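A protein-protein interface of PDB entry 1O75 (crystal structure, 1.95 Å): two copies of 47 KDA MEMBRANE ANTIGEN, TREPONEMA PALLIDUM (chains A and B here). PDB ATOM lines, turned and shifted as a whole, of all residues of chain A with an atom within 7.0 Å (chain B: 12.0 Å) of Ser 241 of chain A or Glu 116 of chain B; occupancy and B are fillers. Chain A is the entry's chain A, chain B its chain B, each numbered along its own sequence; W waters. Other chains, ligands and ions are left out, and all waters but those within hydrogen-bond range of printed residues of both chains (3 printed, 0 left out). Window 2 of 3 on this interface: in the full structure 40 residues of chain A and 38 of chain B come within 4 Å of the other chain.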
ATOM      1  N   LEU A 235      -6.172   5.834  12.794  1.00  0.00           N
ATOM      2  CA  LEU A 235      -7.252   4.982  13.263  1.00  0.00           C
ATOM      3  C   LEU A 235      -7.196   4.643  14.736  1.00  0.00           C
ATOM      4  O   LEU A 235      -6.124   4.641  15.347  1.00  0.00           O
ATOM      5  CB  LEU A 235      -7.216   3.670  12.447  1.00  0.00           C
ATOM      6  CG  LEU A 235      -7.168   3.843  10.915  1.00  0.00           C
ATOM      7  CD1 LEU A 235      -6.703   2.527  10.246  1.00  0.00           C
ATOM      8  CD2 LEU A 235      -8.540   4.236  10.405  1.00  0.00           C
ATOM      9  N   LYS A 236      -8.363   4.355  15.310  1.00  0.00           N
ATOM     10  CA  LYS A 236      -8.445   3.922  16.702  1.00  0.00           C
ATOM     11  C   LYS A 236      -9.583   2.896  16.759  1.00  0.00           C
ATOM     12  O   LYS A 236     -10.287   2.689  15.754  1.00  0.00           O
ATOM     13  CB  LYS A 236      -8.708   5.117  17.641  1.00  0.00           C
ATOM     14  CG  LYS A 236     -10.081   5.792  17.504  1.00  0.00           C
ATOM     15  CD  LYS A 236     -10.181   6.958  18.466  1.00  0.00           C
ATOM     16  CE  LYS A 236     -11.585   7.554  18.489  1.00  0.00           C
ATOM     17  NZ  LYS A 236     -11.603   8.716  19.431  1.00  0.00           N
ATOM     18  N   ARG A 237      -9.757   2.224  17.892  1.00  0.00           N
ATOM     19  CA  ARG A 237     -10.840   1.240  17.973  1.00  0.00           C
ATOM     20  C   ARG A 237     -12.201   1.932  18.208  1.00  0.00           C
ATOM     21  O   ARG A 237     -12.272   3.014  18.811  1.00  0.00           O
ATOM     22  CB  ARG A 237     -10.554   0.205  19.067  1.00  0.00           C
ATOM     23  CG  ARG A 237     -11.097  -1.173  18.722  1.00  0.00           C
ATOM     24  CD  ARG A 237     -10.527  -2.252  19.632  1.00  0.00           C
ATOM     25  NE  ARG A 237     -10.902  -2.043  21.023  1.00  0.00           N
ATOM     26  CZ  ARG A 237     -10.379  -2.721  22.038  1.00  0.00           C
ATOM     27  NH1 ARG A 237      -9.461  -3.654  21.811  1.00  0.00           N
ATOM     28  NH2 ARG A 237     -10.756  -2.452  23.281  1.00  0.00           N
ATOM     29  N   ALA A 238     -13.281   1.326  17.715  1.00  0.00           N
ATOM     30  CA  ALA A 238     -14.608   1.933  17.860  1.00  0.00           C
ATOM     31  C   ALA A 238     -14.938   2.320  19.298  1.00  0.00           C
ATOM     32  O   ALA A 238     -15.611   3.309  19.518  1.00  0.00           O
ATOM     33  CB  ALA A 238     -15.693   0.992  17.306  1.00  0.00           C
ATOM     34  N   ASP A 239     -14.477   1.555  20.283  1.00  0.00           N
ATOM     35  CA  ASP A 239     -14.767   1.915  21.668  1.00  0.00           C
ATOM     36  C   ASP A 239     -13.851   3.020  22.181  1.00  0.00           C
ATOM     37  O   ASP A 239     -13.898   3.373  23.360  1.00  0.00           O
ATOM     38  CB  ASP A 239     -14.640   0.700  22.582  1.00  0.00           C
ATOM     39  CG  ASP A 239     -13.199   0.213  22.712  1.00  0.00           C
ATOM     40  OD1 ASP A 239     -12.334   0.620  21.905  1.00  0.00           O
ATOM     41  OD2 ASP A 239     -12.944  -0.589  23.619  1.00  0.00           O
ATOM     42  N   GLY A 240     -13.019   3.571  21.304  1.00  0.00           N
ATOM     43  CA  GLY A 240     -12.132   4.641  21.734  1.00  0.00           C
ATOM     44  C   GLY A 240     -10.716   4.228  22.131  1.00  0.00           C
ATOM     45  O   GLY A 240      -9.834   5.081  22.195  1.00  0.00           O
ATOM     46  N   SER A 241     -10.487   2.942  22.398  1.00  0.00           N
ATOM     47  CA  SER A 241      -9.149   2.469  22.783  1.00  0.00           C
ATOM     48  C   SER A 241      -8.162   2.675  21.630  1.00  0.00           C
ATOM     49  O   SER A 241      -8.547   2.619  20.460  1.00  0.00           O
ATOM     50  CB  SER A 241      -9.187   0.973  23.115  1.00  0.00           C
ATOM     51  OG  SER A 241     -10.122   0.711  24.151  1.00  0.00           O
ATOM     52  N   GLU A 242      -6.889   2.903  21.939  1.00  0.00           N
ATOM     53  CA  GLU A 242      -5.933   3.056  20.850  1.00  0.00           C
ATOM     54  C   GLU A 242      -5.625   1.637  20.416  1.00  0.00           C
ATOM     55  O   GLU A 242      -5.700   0.706  21.222  1.00  0.00           O
ATOM     56  CB  GLU A 242      -4.647   3.779  21.294  1.00  0.00           C
ATOM     57  CG  GLU A 242      -3.698   2.956  22.123  1.00  0.00           C
ATOM     58  CD  GLU A 242      -2.342   3.658  22.398  1.00  0.00           C
ATOM     59  OE1 GLU A 242      -1.625   3.142  23.276  1.00  0.00           O
ATOM     60  OE2 GLU A 242      -2.005   4.697  21.769  1.00  0.00           O
ATOM     61  N   LEU A 243      -5.297   1.469  19.138  1.00  0.00           N
ATOM     62  CA  LEU A 243      -4.998   0.159  18.597  1.00  0.00           C
ATOM     63  C   LEU A 243      -3.618  -0.381  18.959  1.00  0.00           C
ATOM     64  O   LEU A 243      -2.651   0.372  19.028  1.00  0.00           O
ATOM     65  CB  LEU A 243      -5.094   0.208  17.071  1.00  0.00           C
ATOM     66  CG  LEU A 243      -6.462   0.603  16.512  1.00  0.00           C
ATOM     67  CD1 LEU A 243      -6.326   0.971  15.043  1.00  0.00           C
ATOM     68  CD2 LEU A 243      -7.437  -0.562  16.705  1.00  0.00           C
ATOM     69  N   SER A 244      -3.540  -1.688  19.170  1.00  0.00           N
ATOM     70  CA  SER A 244      -2.266  -2.346  19.431  1.00  0.00           C
ATOM     71  C   SER A 244      -1.682  -2.580  18.031  1.00  0.00           C
ATOM     72  O   SER A 244      -2.391  -2.473  17.016  1.00  0.00           O
ATOM     73  CB  SER A 244      -2.483  -3.703  20.108  1.00  0.00           C
ATOM     74  OG  SER A 244      -3.077  -4.622  19.196  1.00  0.00           O
ATOM     75  N   GLU A 247      -3.635  -5.303  16.313  1.00  0.00           N
ATOM     76  CA  GLU A 247      -4.963  -4.911  15.834  1.00  0.00           C
ATOM     77  C   GLU A 247      -4.843  -4.104  14.543  1.00  0.00           C
ATOM     78  O   GLU A 247      -5.643  -4.277  13.635  1.00  0.00           O
ATOM     79  CB  GLU A 247      -5.700  -4.105  16.905  1.00  0.00           C
ATOM     80  CG  GLU A 247      -6.110  -4.959  18.097  1.00  0.00           C
ATOM     81  CD  GLU A 247      -6.596  -4.138  19.258  1.00  0.00           C
ATOM     82  OE1 GLU A 247      -6.016  -3.062  19.514  1.00  0.00           O
ATOM     83  OE2 GLU A 247      -7.552  -4.565  19.932  1.00  0.00           O
ATOM     84  N   PHE B 111       3.356  10.880  37.024  1.00  0.00           N
ATOM     85  CA  PHE B 111       2.824   9.922  36.067  1.00  0.00           C
ATOM     86  C   PHE B 111       2.110   8.763  36.751  1.00  0.00           C
ATOM     87  O   PHE B 111       2.659   8.137  37.657  1.00  0.00           O
ATOM     88  CB  PHE B 111       3.957   9.361  35.196  1.00  0.00           C
ATOM     89  CG  PHE B 111       3.515   8.253  34.286  1.00  0.00           C
ATOM     90  CD1 PHE B 111       2.716   8.526  33.177  1.00  0.00           C
ATOM     91  CD2 PHE B 111       3.868   6.936  34.559  1.00  0.00           C
ATOM     92  CE1 PHE B 111       2.271   7.492  32.351  1.00  0.00           C
ATOM     93  CE2 PHE B 111       3.435   5.895  33.753  1.00  0.00           C
ATOM     94  CZ  PHE B 111       2.629   6.171  32.638  1.00  0.00           C
ATOM     95  N   GLN B 112       0.898   8.463  36.292  1.00  0.00           N
ATOM     96  CA  GLN B 112       0.110   7.358  36.853  1.00  0.00           C
ATOM     97  C   GLN B 112       0.080   6.172  35.891  1.00  0.00           C
ATOM     98  O   GLN B 112       0.415   5.056  36.274  1.00  0.00           O
ATOM     99  CB  GLN B 112      -1.339   7.799  37.161  1.00  0.00           C
ATOM    100  CG  GLN B 112      -1.470   8.874  38.240  1.00  0.00           C
ATOM    101  CD  GLN B 112      -0.701   8.539  39.520  1.00  0.00           C
ATOM    102  OE1 GLN B 112       0.272   9.220  39.874  1.00  0.00           O
ATOM    103  NE2 GLN B 112      -1.129   7.488  40.219  1.00  0.00           N
ATOM    104  N   ASP B 113      -0.312   6.402  34.641  1.00  0.00           N
ATOM    105  CA  ASP B 113      -0.354   5.313  33.673  1.00  0.00           C
ATOM    106  C   ASP B 113      -0.773   5.762  32.280  1.00  0.00           C
ATOM    107  O   ASP B 113      -1.191   6.907  32.074  1.00  0.00           O
ATOM    108  CB  ASP B 113      -1.324   4.228  34.160  1.00  0.00           C
ATOM    109  CG  ASP B 113      -2.704   4.791  34.493  1.00  0.00           C
ATOM    110  OD1 ASP B 113      -3.451   5.129  33.551  1.00  0.00           O
ATOM    111  OD2 ASP B 113      -3.043   4.912  35.698  1.00  0.00           O
ATOM    112  N   LEU B 114      -0.657   4.856  31.315  1.00  0.00           N
ATOM    113  CA  LEU B 114      -1.091   5.172  29.959  1.00  0.00           C
ATOM    114  C   LEU B 114      -2.516   4.624  29.847  1.00  0.00           C
ATOM    115  O   LEU B 114      -2.726   3.427  30.016  1.00  0.00           O
ATOM    116  CB  LEU B 114      -0.197   4.494  28.911  1.00  0.00           C
ATOM    117  CG  LEU B 114      -0.594   4.815  27.469  1.00  0.00           C
ATOM    118  CD1 LEU B 114      -0.316   6.285  27.173  1.00  0.00           C
ATOM    119  CD2 LEU B 114       0.174   3.927  26.521  1.00  0.00           C
ATOM    120  N   GLY B 115      -3.485   5.499  29.577  1.00  0.00           N
ATOM    121  CA  GLY B 115      -4.867   5.068  29.448  1.00  0.00           C
ATOM    122  C   GLY B 115      -5.079   4.168  28.240  1.00  0.00           C
ATOM    123  O   GLY B 115      -4.263   4.162  27.314  1.00  0.00           O
ATOM    124  N   GLU B 116      -6.174   3.407  28.250  1.00  0.00           N
ATOM    125  CA  GLU B 116      -6.518   2.502  27.151  1.00  0.00           C
ATOM    126  C   GLU B 116      -6.670   3.292  25.862  1.00  0.00           C
ATOM    127  O   GLU B 116      -6.438   2.771  24.766  1.00  0.00           O
ATOM    128  CB  GLU B 116      -7.831   1.770  27.449  1.00  0.00           C
ATOM    129  CG  GLU B 116      -7.738   0.768  28.589  1.00  0.00           C
ATOM    130  CD  GLU B 116      -6.961  -0.482  28.210  1.00  0.00           C
ATOM    131  OE1 GLU B 116      -7.435  -1.224  27.321  1.00  0.00           O
ATOM    132  OE2 GLU B 116      -5.878  -0.727  28.797  1.00  0.00           O
ATOM    133  N   ASP B 117      -7.062   4.552  26.012  1.00  0.00           N
ATOM    134  CA  ASP B 117      -7.241   5.460  24.892  1.00  0.00           C
ATOM    135  C   ASP B 117      -5.931   6.082  24.412  1.00  0.00           C
ATOM    136  O   ASP B 117      -5.933   6.923  23.521  1.00  0.00           O
ATOM    137  CB  ASP B 117      -8.228   6.570  25.266  1.00  0.00           C
ATOM    138  CG  ASP B 117      -7.718   7.475  26.391  1.00  0.00           C
ATOM    139  OD1 ASP B 117      -6.641   7.211  26.971  1.00  0.00           O
ATOM    140  OD2 ASP B 117      -8.423   8.463  26.691  1.00  0.00           O
ATOM    141  N   GLY B 118      -4.816   5.662  25.004  1.00  0.00           N
ATOM    142  CA  GLY B 118      -3.529   6.192  24.599  1.00  0.00           C
ATOM    143  C   GLY B 118      -3.157   7.527  25.207  1.00  0.00           C
ATOM    144  O   GLY B 118      -2.170   8.126  24.800  1.00  0.00           O
ATOM    145  N   GLU B 119      -3.938   8.015  26.166  1.00  0.00           N
ATOM    146  CA  GLU B 119      -3.604   9.292  26.778  1.00  0.00           C
ATOM    147  C   GLU B 119      -2.857   9.093  28.103  1.00  0.00           C
ATOM    148  O   GLU B 119      -3.120   8.155  28.867  1.00  0.00           O
ATOM    149  CB  GLU B 119      -4.867  10.133  26.996  1.00  0.00           C
ATOM    150  CG  GLU B 119      -5.581  10.528  25.688  1.00  0.00           C
ATOM    151  CD  GLU B 119      -4.750  11.471  24.810  1.00  0.00           C
ATOM    152  OE1 GLU B 119      -4.340  12.550  25.292  1.00  0.00           O
ATOM    153  OE2 GLU B 119      -4.513  11.143  23.629  1.00  0.00           O
ATOM    154  N   ILE B 120      -1.914   9.981  28.367  1.00  0.00           N
ATOM    155  CA  ILE B 120      -1.134   9.883  29.578  1.00  0.00           C
ATOM    156  C   ILE B 120      -1.928  10.417  30.759  1.00  0.00           C
ATOM    157  O   ILE B 120      -2.401  11.540  30.736  1.00  0.00           O
ATOM    158  CB  ILE B 120       0.197  10.641  29.393  1.00  0.00           C
ATOM    159  CG1 ILE B 120       1.031   9.901  28.329  1.00  0.00           C
ATOM    160  CG2 ILE B 120       0.973  10.682  30.709  1.00  0.00           C
ATOM    161  CD1 ILE B 120       2.044  10.765  27.628  1.00  0.00           C
ATOM    162  N   LYS B 121      -2.086   9.590  31.786  1.00  0.00           N
ATOM    163  CA  LYS B 121      -2.829   9.987  32.973  1.00  0.00           C
ATOM    164  C   LYS B 121      -1.814  10.339  34.045  1.00  0.00           C
ATOM    165  O   LYS B 121      -0.811   9.631  34.226  1.00  0.00           O
ATOM    166  CB  LYS B 121      -3.728   8.836  33.429  1.00  0.00           C
ATOM    167  CG  LYS B 121      -4.610   8.320  32.282  1.00  0.00           C
ATOM    168  CD  LYS B 121      -5.383   9.496  31.672  1.00  0.00           C
ATOM    169  CE  LYS B 121      -5.926   9.225  30.263  1.00  0.00           C
ATOM    170  NZ  LYS B 121      -6.768   8.001  30.172  1.00  0.00           N
ATOM    171  N   PHE B 122      -2.070  11.420  34.764  1.00  0.00           N
ATOM    172  CA  PHE B 122      -1.126  11.840  35.783  1.00  0.00           C
ATOM    173  C   PHE B 122      -1.838  12.750  36.751  1.00  0.00           C
ATOM    174  O   PHE B 122      -2.981  13.140  36.510  1.00  0.00           O
ATOM    175  CB  PHE B 122       0.014  12.615  35.108  1.00  0.00           C
ATOM    176  CG  PHE B 122      -0.462  13.780  34.275  1.00  0.00           C
ATOM    177  CD1 PHE B 122      -0.782  14.999  34.868  1.00  0.00           C
ATOM    178  CD2 PHE B 122      -0.638  13.648  32.905  1.00  0.00           C
ATOM    179  CE1 PHE B 122      -1.272  16.070  34.102  1.00  0.00           C
ATOM    180  CE2 PHE B 122      -1.126  14.712  32.136  1.00  0.00           C
ATOM    181  CZ  PHE B 122      -1.444  15.922  32.738  1.00  0.00           C
ATOM    182  N   SER B 244       4.865  -2.855  23.730  1.00  0.00           N
ATOM    183  CA  SER B 244       3.548  -2.266  23.523  1.00  0.00           C
ATOM    184  C   SER B 244       3.753  -0.774  23.814  1.00  0.00           C
ATOM    185  O   SER B 244       4.764  -0.396  24.423  1.00  0.00           O
ATOM    186  CB  SER B 244       2.549  -2.844  24.534  1.00  0.00           C
ATOM    187  OG  SER B 244       2.838  -2.410  25.863  1.00  0.00           O
ATOM    188  N   HIS B 245       2.804   0.070  23.410  1.00  0.00           N
ATOM    189  CA  HIS B 245       2.911   1.515  23.647  1.00  0.00           C
ATOM    190  C   HIS B 245       3.021   1.716  25.156  1.00  0.00           C
ATOM    191  O   HIS B 245       3.838   2.507  25.639  1.00  0.00           O
ATOM    192  CB  HIS B 245       1.658   2.232  23.091  1.00  0.00           C
ATOM    193  CG  HIS B 245       1.753   3.730  23.059  1.00  0.00           C
ATOM    194  ND1 HIS B 245       0.642   4.539  22.912  1.00  0.00           N
ATOM    195  CD2 HIS B 245       2.818   4.569  23.117  1.00  0.00           C
ATOM    196  CE1 HIS B 245       1.016   5.806  22.882  1.00  0.00           C
ATOM    197  NE2 HIS B 245       2.333   5.854  23.006  1.00  0.00           N
ATOM    198  N   ARG B 246       2.225   0.967  25.910  1.00  0.00           N
ATOM    199  CA  ARG B 246       2.259   1.096  27.359  1.00  0.00           C
ATOM    200  C   ARG B 246       3.619   0.716  27.965  1.00  0.00           C
ATOM    201  O   ARG B 246       4.107   1.381  28.877  1.00  0.00           O
ATOM    202  CB  ARG B 246       1.152   0.247  27.991  1.00  0.00           C
ATOM    203  CG  ARG B 246       1.257   0.137  29.503  1.00  0.00           C
ATOM    204  CD  ARG B 246      -0.120   0.142  30.139  1.00  0.00           C
ATOM    205  NE  ARG B 246      -1.047  -0.670  29.361  1.00  0.00           N
ATOM    206  CZ  ARG B 246      -2.370  -0.542  29.395  1.00  0.00           C
ATOM    207  NH1 ARG B 246      -2.934   0.370  30.181  1.00  0.00           N
ATOM    208  NH2 ARG B 246      -3.129  -1.309  28.619  1.00  0.00           N
ATOM    209  N   GLU B 247       4.231  -0.347  27.466  1.00  0.00           N
ATOM    210  CA  GLU B 247       5.535  -0.741  28.006  1.00  0.00           C
ATOM    211  C   GLU B 247       6.608   0.316  27.703  1.00  0.00           C
ATOM    212  O   GLU B 247       7.471   0.578  28.529  1.00  0.00           O
ATOM    213  CB  GLU B 247       5.949  -2.120  27.465  1.00  0.00           C
ATOM    214  CG  GLU B 247       5.104  -3.279  28.071  1.00  0.00           C
ATOM    215  CD  GLU B 247       5.312  -4.596  27.342  1.00  0.00           C
ATOM    216  OE1 GLU B 247       5.579  -4.575  26.121  1.00  0.00           O
ATOM    217  OE2 GLU B 247       5.197  -5.659  27.979  1.00  0.00           O
ATOM    218  N   ILE B 249       6.055   3.583  27.213  1.00  0.00           N
ATOM    219  CA  ILE B 249       5.776   4.750  28.030  1.00  0.00           C
ATOM    220  C   ILE B 249       6.245   4.554  29.479  1.00  0.00           C
ATOM    221  O   ILE B 249       6.790   5.472  30.090  1.00  0.00           O
ATOM    222  CB  ILE B 249       4.264   5.089  27.966  1.00  0.00           C
ATOM    223  CG1 ILE B 249       3.951   5.636  26.576  1.00  0.00           C
ATOM    224  CG2 ILE B 249       3.888   6.117  29.029  1.00  0.00           C
ATOM    225  CD1 ILE B 249       4.747   6.874  26.221  1.00  0.00           C
ATOM    226  N   ASP B 250       6.033   3.364  30.036  1.00  0.00           N
ATOM    227  CA  ASP B 250       6.465   3.116  31.411  1.00  0.00           C
ATOM    228  C   ASP B 250       7.983   3.322  31.486  1.00  0.00           C
ATOM    229  O   ASP B 250       8.507   3.830  32.472  1.00  0.00           O
ATOM    230  CB  ASP B 250       6.130   1.684  31.854  1.00  0.00           C
ATOM    231  CG  ASP B 250       4.652   1.499  32.200  1.00  0.00           C
ATOM    232  OD1 ASP B 250       3.966   2.502  32.500  1.00  0.00           O
ATOM    233  OD2 ASP B 250       4.172   0.344  32.197  1.00  0.00           O
ATOM    234  N   THR B 288       6.410  10.575  23.006  1.00  0.00           N
ATOM    235  CA  THR B 288       5.443   9.706  23.675  1.00  0.00           C
ATOM    236  C   THR B 288       4.647   8.873  22.676  1.00  0.00           C
ATOM    237  O   THR B 288       3.620   8.279  23.021  1.00  0.00           O
ATOM    238  CB  THR B 288       4.465  10.541  24.499  1.00  0.00           C
ATOM    239  OG1 THR B 288       3.821  11.480  23.636  1.00  0.00           O
ATOM    240  CG2 THR B 288       5.192  11.282  25.579  1.00  0.00           C
ATOM    241  N   ARG B 290       4.301   5.842  19.506  1.00  0.00           N
ATOM    242  CA  ARG B 290       4.389   4.392  19.526  1.00  0.00           C
ATOM    243  C   ARG B 290       5.748   3.777  19.200  1.00  0.00           C
ATOM    244  O   ARG B 290       5.956   2.602  19.474  1.00  0.00           O
ATOM    245  CB  ARG B 290       3.336   3.829  18.577  1.00  0.00           C
ATOM    246  CG  ARG B 290       1.906   4.156  19.005  1.00  0.00           C
ATOM    247  CD  ARG B 290       1.026   4.229  17.799  1.00  0.00           C
ATOM    248  NE  ARG B 290      -0.391   4.153  18.139  1.00  0.00           N
ATOM    249  CZ  ARG B 290      -0.954   3.110  18.740  1.00  0.00           C
ATOM    250  NH1 ARG B 290      -0.218   2.052  19.084  1.00  0.00           N
ATOM    251  NH2 ARG B 290      -2.259   3.112  18.964  1.00  0.00           N
HETATM  252  O   HOH W   1      -5.108   0.390  24.538  1.00  0.00           O
HETATM  253  O   HOH W   2      -7.505   6.432  21.226  1.00  0.00           O
HETATM  254  O   HOH W   3      -4.987   3.976  17.742  1.00  0.00           O
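N of Glu 242 of chain A lies within hydrogen-bond range of O of Glu 116 of chain B, 2.9 Å away.
OE1 of Glu 242 of chain A is in hydrogen-bond range of ND1 of His 245 of chain B.
NH2 of Arg 290 of chain B is in salt-bridge range of OE2 of Glu 242 of chain A.
The backbone carbonyl oxygen of Leu 243 of chain A lies within hydrogen-bond range of the guanidinium group of Arg 290 of chain B (2.8 Å).
NH2 of Arg 237 of chain A sits at hydrogen-bond distance from OG of Ser 241 of chain A (3.3 Å).
The side-chain carboxylate of Asp 239 of chain A lies within hydrogen-bond range of the backbone NH of Ser 241 of chain A, 3.0 Å away.
The guanidinium group (NH2) of Arg 246 of chain B is in salt-bridge range of the side-chain carboxylate (OE2) of Glu 116 of chain B (2.8 Å).
The side-chain carboxylate (OD1) of Asp 117 of chain B is in hydrogen-bond range of the backbone NH (N) of Glu 119 of chain B.
The side-chain carboxylate of Asp 117 of chain B is in salt-bridge range of the side-chain amino group of Lys 121 of chain B.
NE2 of His 245 of chain B is in hydrogen-bond range of O of Thr 288 of chain B.
Gly 240 of chain A touches Asp 117 of chain B.
O of Glu 116 of chain B touches CA of Ser 241 of chain A, 3.4 Å away.
Glu 242 of chain A touches Leu 114 of chain B (OE1 to CD2, 3.8 Å).
Glu 242 of chain A touches Asp 117 of chain B.
CA of Gly 118 of chain B touches OE2 of Glu 242 of chain A (3.5 Å).
No residue of chain B comes within 4 Å of Lys 236 of chain A.
No residue of chain B comes within 4 Å of Ala 238 of chain A.
No residue of chain B comes within 4 Å of Asp 239 of chain A.
Printed residues of chain B within 4 Å of Gly 240 of chain A: Asp 117 (3.8 Å).
Ser 241 of chain A touches one residue of chain B.
Glu 242 of chain A touches six residues of chain B.
Gln 112 of chain B touches none of the printed residues of chain A.
Of the printed residues of chain A, Leu 114 of chain B touches Glu 242.
Of the printed residues of chain A, Glu 116 of chain B touches Ser 241 (3.4 Å) and Glu 242 (2.9 Å).
Printed residues of chain A within 4 Å of Asp 117 of chain B: Gly 240 (3.8 Å) and Glu 242 (3.9 Å).
Of the printed residues of chain A, Gly 118 of chain B touches Glu 242 (3.5 Å).
Ser 244 of chain B touches none of the printed residues of chain A.
Of the printed residues of chain A, His 245 of chain B touches Glu 242.
Printed residues of chain A within 4 Å of Arg 290 of chain B: Glu 242 and Leu 243.
The nearest residue of chain B that does not touch Ser 241 of chain A is Asp 117 of chain B (4.1 Å).
Printed residues of chain B that touch a printed residue of chain A: Leu 114, Glu 116, Asp 117, Gly 118, His 245 and Arg 290.
Hydrophobic or aromatic side chains of chain B within 4 Å of the printed part of chain A: Leu 114 and His 245.
Among the printed residues, 9 pairs touch across the chains.
Among the printed residues, Asp or Glu carboxylates within 4 Å of a Lys or Arg side-chain nitrogen of the other chain: Glu 242 of chain A with Arg 290 of chain B (3.2 Å).
Positions printed for both chains: 244 and 247.
Of the 9 pairs that touch across the chains among the printed residues, none has its exchanged pair printed and touching as well.
Water W3 lies within hydrogen-bond range of O of Leu 235 of chain A (2.7 Å), N of Leu 243 of chain A (2.9 Å) and NH2 of Arg 290 of chain B (3.1 Å).
Water W1 bridges the backbone carbonyl oxygen of Glu 116 of chain B (2.7 Å) and the backbone carbonyl oxygen of Glu 242 of chain A (3.4 Å).
Water W2 lies within hydrogen-bond range of the backbone carbonyl oxygen (O) of Asp 117 of chain B and the backbone carbonyl oxygen (O) of Gly 240 of chain A.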
